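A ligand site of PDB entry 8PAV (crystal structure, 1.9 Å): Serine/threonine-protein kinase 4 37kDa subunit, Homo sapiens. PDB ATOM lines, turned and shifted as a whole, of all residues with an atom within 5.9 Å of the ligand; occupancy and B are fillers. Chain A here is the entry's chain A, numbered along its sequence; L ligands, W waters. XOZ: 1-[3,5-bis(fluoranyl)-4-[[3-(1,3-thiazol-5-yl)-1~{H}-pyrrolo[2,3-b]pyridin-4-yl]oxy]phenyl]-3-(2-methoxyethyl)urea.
O of Glu 104 sits at hydrogen-bond distance from N4 of the ligand, at 2.5 Å.
N16 of the ligand lies within hydrogen-bond range of OD2 of Asp 113 (2.8 Å).
N6 of the ligand is in hydrogen-bond range of N of Cys 106, at 2.9 Å.
The guanidinium group (NH1) of Arg 116 sits at hydrogen-bond distance from an oxygen (O21) of the ligand, 3.3 Å away.
OD1 of Asp 113 lies within salt-bridge range of NH1 of Arg 116, 2.9 Å away.
N of Asp 113 lies within hydrogen-bond range of OG of Ser 110, 2.9 Å away.
O of Val 45 is in hydrogen-bond range of N of Leu 37, at 2.8 Å.
O of Gly 38 is in hydrogen-bond range of N of Val 45, at 3.3 Å.
The backbone NH of Met 103 lies within hydrogen-bond range of the backbone carbonyl oxygen of Ala 58 (2.8 Å).
O of Leu 37 sits close to O23 of the ligand.
The side-chain sulfur of Met 103 lies close to a sulfur (S31) of the ligand.
Merely in contact with the ligand: Leu 157 (3.1 Å), Val 45 (3.1 Å), Ala 58 (3.5 Å), Gly 38 (3.7 Å), Tyr 105 (3.8 Å) and Val 87 (3.8 Å).
Hydrophobic or aromatic side chains that line the ligand: Leu 37, Val 45, Ala 58, Val 87, Met 103, Tyr 105 and Leu 157.
12 residues have an atom within 4 Å of the ligand: Leu 37, Gly 38, Val 45, Ala 58, Val 87, Met 103, Glu 104, Tyr 105, Cys 106, Asp 113, Arg 116 and Leu 157.
The nearest printed residue that does not touch the ligand is Lys 60 (4.2 Å).
Water W1 lies within hydrogen-bond range of OE1 of Glu 74, NZ of Lys 60 and N29 of the ligand.
Water W2 lies within hydrogen-bond range of S31 of the ligand (2.9 Å), N of Asp 168 (3.3 Å) and SD of Met 78 (3.3 Å).
Water W3 lies within hydrogen-bond range of N29 of the ligand (3.0 Å) and NZ of Lys 60 (3.5 Å).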
ATOM      1  N   LEU A  37      -7.788  10.778 -17.811  1.00  0.00           N
ATOM      2  CA  LEU A  37      -8.552   9.534 -17.514  1.00  0.00           C
ATOM      3  C   LEU A  37      -8.578   8.621 -18.760  1.00  0.00           C
ATOM      4  O   LEU A  37      -8.805   7.412 -18.582  1.00  0.00           O
ATOM      5  CB  LEU A  37      -9.984   9.875 -17.119  1.00  0.00           C
ATOM      6  CG  LEU A  37     -10.184  10.718 -15.855  1.00  0.00           C
ATOM      7  CD1 LEU A  37     -11.638  11.126 -15.714  1.00  0.00           C
ATOM      8  CD2 LEU A  37      -9.717   9.958 -14.622  1.00  0.00           C
ATOM      9  N   GLY A  38      -8.419   9.176 -19.971  1.00  0.00           N
ATOM     10  CA  GLY A  38      -8.609   8.461 -21.243  1.00  0.00           C
ATOM     11  C   GLY A  38      -7.940   9.193 -22.395  1.00  0.00           C
ATOM     12  O   GLY A  38      -7.573  10.365 -22.197  1.00  0.00           O
ATOM     13  N   GLU A  39      -7.786   8.529 -23.555  1.00  0.00           N
ATOM     14  CA  GLU A  39      -6.975   9.040 -24.696  1.00  0.00           C
ATOM     15  C   GLU A  39      -7.253   8.269 -25.993  1.00  0.00           C
ATOM     16  O   GLU A  39      -8.212   7.457 -26.012  1.00  0.00           O
ATOM     17  CB  GLU A  39      -5.489   8.920 -24.342  1.00  0.00           C
ATOM     18  CG  GLU A  39      -4.594   9.793 -25.207  1.00  0.00           C
ATOM     19  CD  GLU A  39      -3.249  10.108 -24.554  1.00  0.00           C
ATOM     20  OE1 GLU A  39      -2.772   9.263 -23.761  1.00  0.00           O
ATOM     21  OE2 GLU A  39      -2.690  11.192 -24.827  1.00  0.00           O
ATOM     22  N   GLY A  43     -12.278  10.477 -27.746  1.00  0.00           N
ATOM     23  CA  GLY A  43     -11.376  11.627 -27.528  1.00  0.00           C
ATOM     24  C   GLY A  43     -10.627  11.534 -26.204  1.00  0.00           C
ATOM     25  O   GLY A  43     -10.561  10.429 -25.610  1.00  0.00           O
ATOM     26  N   VAL A  45      -9.973  12.652 -22.241  1.00  0.00           N
ATOM     27  CA  VAL A  45     -10.853  12.908 -21.060  1.00  0.00           C
ATOM     28  C   VAL A  45      -9.974  13.185 -19.833  1.00  0.00           C
ATOM     29  O   VAL A  45      -8.982  12.455 -19.640  1.00  0.00           O
ATOM     30  CB  VAL A  45     -11.806  11.723 -20.828  1.00  0.00           C
ATOM     31  CG1 VAL A  45     -12.805  12.017 -19.715  1.00  0.00           C
ATOM     32  CG2 VAL A  45     -12.534  11.346 -22.109  1.00  0.00           C
ATOM     33  N   ALA A  58     -15.738  15.256 -15.229  1.00  0.00           N
ATOM     34  CA  ALA A  58     -14.919  14.726 -16.350  1.00  0.00           C
ATOM     35  C   ALA A  58     -15.043  15.725 -17.504  1.00  0.00           C
ATOM     36  O   ALA A  58     -16.164  16.187 -17.777  1.00  0.00           O
ATOM     37  CB  ALA A  58     -15.384  13.344 -16.755  1.00  0.00           C
ATOM     38  N   LYS A  60     -14.132  16.068 -21.478  1.00  0.00           N
ATOM     39  CA  LYS A  60     -13.641  15.507 -22.766  1.00  0.00           C
ATOM     40  C   LYS A  60     -13.154  16.674 -23.615  1.00  0.00           C
ATOM     41  O   LYS A  60     -13.936  17.623 -23.786  1.00  0.00           O
ATOM     42  CB  LYS A  60     -14.751  14.693 -23.440  1.00  0.00           C
ATOM     43  CG  LYS A  60     -14.392  14.023 -24.770  1.00  0.00           C
ATOM     44  CD  LYS A  60     -15.524  13.127 -25.212  1.00  0.00           C
ATOM     45  CE  LYS A  60     -15.335  12.416 -26.533  1.00  0.00           C
ATOM     46  NZ  LYS A  60     -16.517  11.567 -26.814  1.00  0.00           N
ATOM     47  N   GLU A  74     -24.142  12.808 -29.303  1.00  0.00           N
ATOM     48  CA  GLU A  74     -24.150  12.294 -27.917  1.00  0.00           C
ATOM     49  C   GLU A  74     -24.503  13.438 -26.965  1.00  0.00           C
ATOM     50  O   GLU A  74     -25.286  13.208 -26.019  1.00  0.00           O
ATOM     51  CB  GLU A  74     -22.849  11.601 -27.520  1.00  0.00           C
ATOM     52  CG  GLU A  74     -21.626  12.483 -27.343  1.00  0.00           C
ATOM     53  CD  GLU A  74     -20.410  11.650 -26.929  1.00  0.00           C
ATOM     54  OE1 GLU A  74     -20.592  10.670 -26.182  1.00  0.00           O
ATOM     55  OE2 GLU A  74     -19.296  11.960 -27.357  1.00  0.00           O
ATOM     56  N   MET A  78     -27.681  13.520 -24.321  1.00  0.00           N
ATOM     57  CA  MET A  78     -27.429  13.699 -22.869  1.00  0.00           C
ATOM     58  C   MET A  78     -28.106  14.975 -22.371  1.00  0.00           C
ATOM     59  O   MET A  78     -28.645  14.940 -21.250  1.00  0.00           O
ATOM     60  CB  MET A  78     -25.938  13.754 -22.553  1.00  0.00           C
ATOM     61  CG  MET A  78     -25.280  12.409 -22.620  1.00  0.00           C
ATOM     62  SD  MET A  78     -23.518  12.545 -22.140  1.00  0.00           S
ATOM     63  CE  MET A  78     -22.867  13.234 -23.657  1.00  0.00           C
ATOM     64  N   VAL A  87     -25.426   9.334 -17.563  1.00  0.00           N
ATOM     65  CA  VAL A  87     -24.322  10.319 -17.371  1.00  0.00           C
ATOM     66  C   VAL A  87     -24.848  11.715 -17.729  1.00  0.00           C
ATOM     67  O   VAL A  87     -25.412  11.900 -18.818  1.00  0.00           O
ATOM     68  CB  VAL A  87     -23.063   9.956 -18.187  1.00  0.00           C
ATOM     69  CG1 VAL A  87     -22.003  11.047 -18.088  1.00  0.00           C
ATOM     70  CG2 VAL A  87     -22.486   8.638 -17.732  1.00  0.00           C
ATOM     71  N   MET A 103     -18.844  16.811 -18.102  1.00  0.00           N
ATOM     72  CA  MET A 103     -19.811  15.740 -17.795  1.00  0.00           C
ATOM     73  C   MET A 103     -19.617  15.234 -16.371  1.00  0.00           C
ATOM     74  O   MET A 103     -18.551  15.470 -15.745  1.00  0.00           O
ATOM     75  CB  MET A 103     -19.629  14.563 -18.755  1.00  0.00           C
ATOM     76  CG  MET A 103     -19.934  14.911 -20.206  1.00  0.00           C
ATOM     77  SD  MET A 103     -19.513  13.508 -21.257  1.00  0.00           S
ATOM     78  CE  MET A 103     -17.731  13.483 -21.183  1.00  0.00           C
ATOM     79  N   GLU A 104     -20.632  14.503 -15.909  1.00  0.00           N
ATOM     80  CA  GLU A 104     -20.649  13.822 -14.610  1.00  0.00           C
ATOM     81  C   GLU A 104     -19.435  12.890 -14.538  1.00  0.00           C
ATOM     82  O   GLU A 104     -19.224  12.144 -15.532  1.00  0.00           O
ATOM     83  CB  GLU A 104     -21.936  13.022 -14.486  1.00  0.00           C
ATOM     84  CG  GLU A 104     -22.065  12.302 -13.169  1.00  0.00           C
ATOM     85  CD  GLU A 104     -23.409  11.620 -13.060  1.00  0.00           C
ATOM     86  OE1 GLU A 104     -24.153  11.553 -14.076  1.00  0.00           O
ATOM     87  OE2 GLU A 104     -23.678  11.143 -11.981  1.00  0.00           O
ATOM     88  N   TYR A 105     -18.717  12.924 -13.421  1.00  0.00           N
ATOM     89  CA  TYR A 105     -17.510  12.101 -13.188  1.00  0.00           C
ATOM     90  C   TYR A 105     -17.918  10.731 -12.635  1.00  0.00           C
ATOM     91  O   TYR A 105     -18.623  10.675 -11.625  1.00  0.00           O
ATOM     92  CB  TYR A 105     -16.554  12.846 -12.250  1.00  0.00           C
ATOM     93  CG  TYR A 105     -15.357  12.037 -11.816  1.00  0.00           C
ATOM     94  CD1 TYR A 105     -14.391  11.665 -12.733  1.00  0.00           C
ATOM     95  CD2 TYR A 105     -15.206  11.656 -10.489  1.00  0.00           C
ATOM     96  CE1 TYR A 105     -13.282  10.930 -12.333  1.00  0.00           C
ATOM     97  CE2 TYR A 105     -14.096  10.924 -10.076  1.00  0.00           C
ATOM     98  CZ  TYR A 105     -13.131  10.569 -11.010  1.00  0.00           C
ATOM     99  OH  TYR A 105     -12.030   9.872 -10.623  1.00  0.00           O
ATOM    100  N   CYS A 106     -17.510   9.657 -13.301  1.00  0.00           N
ATOM    101  CA  CYS A 106     -17.767   8.246 -12.878  1.00  0.00           C
ATOM    102  C   CYS A 106     -16.405   7.595 -12.594  1.00  0.00           C
ATOM    103  O   CYS A 106     -15.795   7.068 -13.510  1.00  0.00           O
ATOM    104  CB  CYS A 106     -18.543   7.508 -13.956  1.00  0.00           C
ATOM    105  SG  CYS A 106     -20.171   8.251 -14.281  1.00  0.00           S
ATOM    106  N   GLY A 107     -15.937   7.720 -11.347  1.00  0.00           N
ATOM    107  CA  GLY A 107     -14.529   7.519 -10.980  1.00  0.00           C
ATOM    108  C   GLY A 107     -14.067   6.074 -11.091  1.00  0.00           C
ATOM    109  O   GLY A 107     -12.845   5.868 -11.224  1.00  0.00           O
ATOM    110  N   GLY A 109     -14.763   4.136 -13.555  1.00  0.00           N
ATOM    111  CA  GLY A 109     -14.689   3.849 -15.003  1.00  0.00           C
ATOM    112  C   GLY A 109     -15.778   2.874 -15.436  1.00  0.00           C
ATOM    113  O   GLY A 109     -16.817   2.761 -14.739  1.00  0.00           O
ATOM    114  N   SER A 110     -15.564   2.197 -16.557  1.00  0.00           N
ATOM    115  CA  SER A 110     -16.551   1.300 -17.192  1.00  0.00           C
ATOM    116  C   SER A 110     -16.527  -0.063 -16.500  1.00  0.00           C
ATOM    117  O   SER A 110     -15.491  -0.452 -15.915  1.00  0.00           O
ATOM    118  CB  SER A 110     -16.315   1.170 -18.675  1.00  0.00           C
ATOM    119  OG  SER A 110     -15.153   0.421 -18.955  1.00  0.00           O
ATOM    120  N   ASP A 113     -13.712  -1.916 -17.972  1.00  0.00           N
ATOM    121  CA  ASP A 113     -12.462  -1.485 -17.287  1.00  0.00           C
ATOM    122  C   ASP A 113     -12.289  -2.277 -15.993  1.00  0.00           C
ATOM    123  O   ASP A 113     -11.187  -2.840 -15.773  1.00  0.00           O
ATOM    124  CB  ASP A 113     -12.446   0.000 -16.909  1.00  0.00           C
ATOM    125  CG  ASP A 113     -12.309   0.979 -18.076  1.00  0.00           C
ATOM    126  OD1 ASP A 113     -11.818   0.546 -19.149  1.00  0.00           O
ATOM    127  OD2 ASP A 113     -12.707   2.167 -17.870  1.00  0.00           O
ATOM    128  N   ARG A 116     -11.317  -5.931 -16.643  1.00  0.00           N
ATOM    129  CA  ARG A 116      -9.895  -5.928 -17.104  1.00  0.00           C
ATOM    130  C   ARG A 116      -8.950  -5.678 -15.922  1.00  0.00           C
ATOM    131  O   ARG A 116      -8.018  -6.465 -15.756  1.00  0.00           O
ATOM    132  CB  ARG A 116      -9.696  -4.889 -18.215  1.00  0.00           C
ATOM    133  CG  ARG A 116      -8.241  -4.726 -18.634  1.00  0.00           C
ATOM    134  CD  ARG A 116      -7.960  -3.763 -19.783  1.00  0.00           C
ATOM    135  NE  ARG A 116      -8.637  -2.473 -19.683  1.00  0.00           N
ATOM    136  CZ  ARG A 116      -8.367  -1.490 -18.810  1.00  0.00           C
ATOM    137  NH1 ARG A 116      -9.098  -0.391 -18.817  1.00  0.00           N
ATOM    138  NH2 ARG A 116      -7.407  -1.633 -17.907  1.00  0.00           N
ATOM    139  N   GLY A 154     -18.622  -1.768 -21.758  1.00  0.00           N
ATOM    140  CA  GLY A 154     -17.756  -0.596 -21.944  1.00  0.00           C
ATOM    141  C   GLY A 154     -18.526   0.713 -21.847  1.00  0.00           C
ATOM    142  O   GLY A 154     -17.872   1.740 -21.686  1.00  0.00           O
ATOM    143  N   LEU A 157     -20.885   2.990 -16.902  1.00  0.00           N
ATOM    144  CA  LEU A 157     -19.864   3.575 -16.014  1.00  0.00           C
ATOM    145  C   LEU A 157     -20.361   3.483 -14.570  1.00  0.00           C
ATOM    146  O   LEU A 157     -21.588   3.565 -14.329  1.00  0.00           O
ATOM    147  CB  LEU A 157     -19.603   5.045 -16.391  1.00  0.00           C
ATOM    148  CG  LEU A 157     -19.292   5.313 -17.862  1.00  0.00           C
ATOM    149  CD1 LEU A 157     -18.871   6.768 -18.035  1.00  0.00           C
ATOM    150  CD2 LEU A 157     -18.226   4.367 -18.402  1.00  0.00           C
ATOM    151  N   ALA A 167     -23.612   5.556 -20.703  1.00  0.00           N
ATOM    152  CA  ALA A 167     -22.730   6.520 -21.395  1.00  0.00           C
ATOM    153  C   ALA A 167     -22.631   6.186 -22.881  1.00  0.00           C
ATOM    154  O   ALA A 167     -23.095   5.137 -23.300  1.00  0.00           O
ATOM    155  CB  ALA A 167     -21.371   6.512 -20.732  1.00  0.00           C
ATOM    156  N   ASP A 168     -21.946   7.047 -23.631  1.00  0.00           N
ATOM    157  CA  ASP A 168     -21.716   7.010 -25.107  1.00  0.00           C
ATOM    158  C   ASP A 168     -23.015   6.868 -25.880  1.00  0.00           C
ATOM    159  O   ASP A 168     -23.359   5.738 -26.303  1.00  0.00           O
ATOM    160  CB  ASP A 168     -20.774   5.919 -25.596  1.00  0.00           C
ATOM    161  CG  ASP A 168     -20.539   6.028 -27.106  1.00  0.00           C
ATOM    162  OD1 ASP A 168     -20.817   7.145 -27.683  1.00  0.00           O
ATOM    163  OD2 ASP A 168     -20.161   4.985 -27.710  1.00  0.00           O
HETATM  164  C5  XOZ L   1     -16.779  10.100 -16.916  1.00  0.00           C
HETATM  165  C7  XOZ L   1     -15.006   9.071 -15.892  1.00  0.00           C
HETATM  166  C8  XOZ L   1     -14.508   8.633 -17.115  1.00  0.00           C
HETATM  167  C15 XOZ L   1     -12.335   5.108 -19.675  1.00  0.00           C
HETATM  168  C17 XOZ L   1     -10.388   3.820 -20.178  1.00  0.00           C
HETATM  169  C20 XOZ L   1      -8.420   1.583 -21.961  1.00  0.00           C
HETATM  170  C22 XOZ L   1      -6.446   0.273 -21.289  1.00  0.00           C
HETATM  171  C24 XOZ L   1     -13.642   5.018 -19.195  1.00  0.00           C
HETATM  172  C28 XOZ L   1     -16.384  10.160 -21.399  1.00  0.00           C
HETATM  173  O21 XOZ L   1      -7.823   0.271 -21.769  1.00  0.00           O
HETATM  174  C19 XOZ L   1      -8.514   2.329 -20.618  1.00  0.00           C
HETATM  175  N18 XOZ L   1      -9.912   2.577 -20.232  1.00  0.00           N
HETATM  176  O23 XOZ L   1      -9.663   4.758 -20.484  1.00  0.00           O
HETATM  177  N16 XOZ L   1     -11.639   3.968 -19.730  1.00  0.00           N
HETATM  178  C25 XOZ L   1     -14.429   6.160 -19.125  1.00  0.00           C
HETATM  179  F26 XOZ L   1     -15.658   6.060 -18.644  1.00  0.00           F
HETATM  180  C14 XOZ L   1     -11.856   6.343 -20.132  1.00  0.00           C
HETATM  181  C12 XOZ L   1     -12.663   7.476 -20.051  1.00  0.00           C
HETATM  182  F13 XOZ L   1     -12.181   8.666 -20.472  1.00  0.00           F
HETATM  183  C11 XOZ L   1     -13.960   7.402 -19.539  1.00  0.00           C
HETATM  184  O10 XOZ L   1     -14.759   8.516 -19.514  1.00  0.00           O
HETATM  185  C9  XOZ L   1     -15.192   8.945 -18.288  1.00  0.00           C
HETATM  186  C1  XOZ L   1     -16.363   9.694 -18.187  1.00  0.00           C
HETATM  187  N6  XOZ L   1     -16.107   9.778 -15.805  1.00  0.00           N
HETATM  188  N4  XOZ L   1     -17.905  10.791 -17.098  1.00  0.00           N
HETATM  189  C3  XOZ L   1     -18.208  10.848 -18.355  1.00  0.00           C
HETATM  190  C2  XOZ L   1     -17.319  10.206 -19.067  1.00  0.00           C
HETATM  191  C27 XOZ L   1     -17.374  10.098 -20.470  1.00  0.00           C
HETATM  192  N29 XOZ L   1     -16.798  10.059 -22.683  1.00  0.00           N
HETATM  193  C30 XOZ L   1     -18.134   9.960 -22.848  1.00  0.00           C
HETATM  194  S31 XOZ L   1     -18.876   9.945 -21.294  1.00  0.00           S
HETATM  195  O   HOH W   1     -18.352   9.300 -25.632  1.00  0.00           O
HETATM  196  O   HOH W   2     -21.670   9.839 -21.966  1.00  0.00           O
HETATM  197  O   HOH W   3     -14.645   9.571 -24.689  1.00  0.00           O
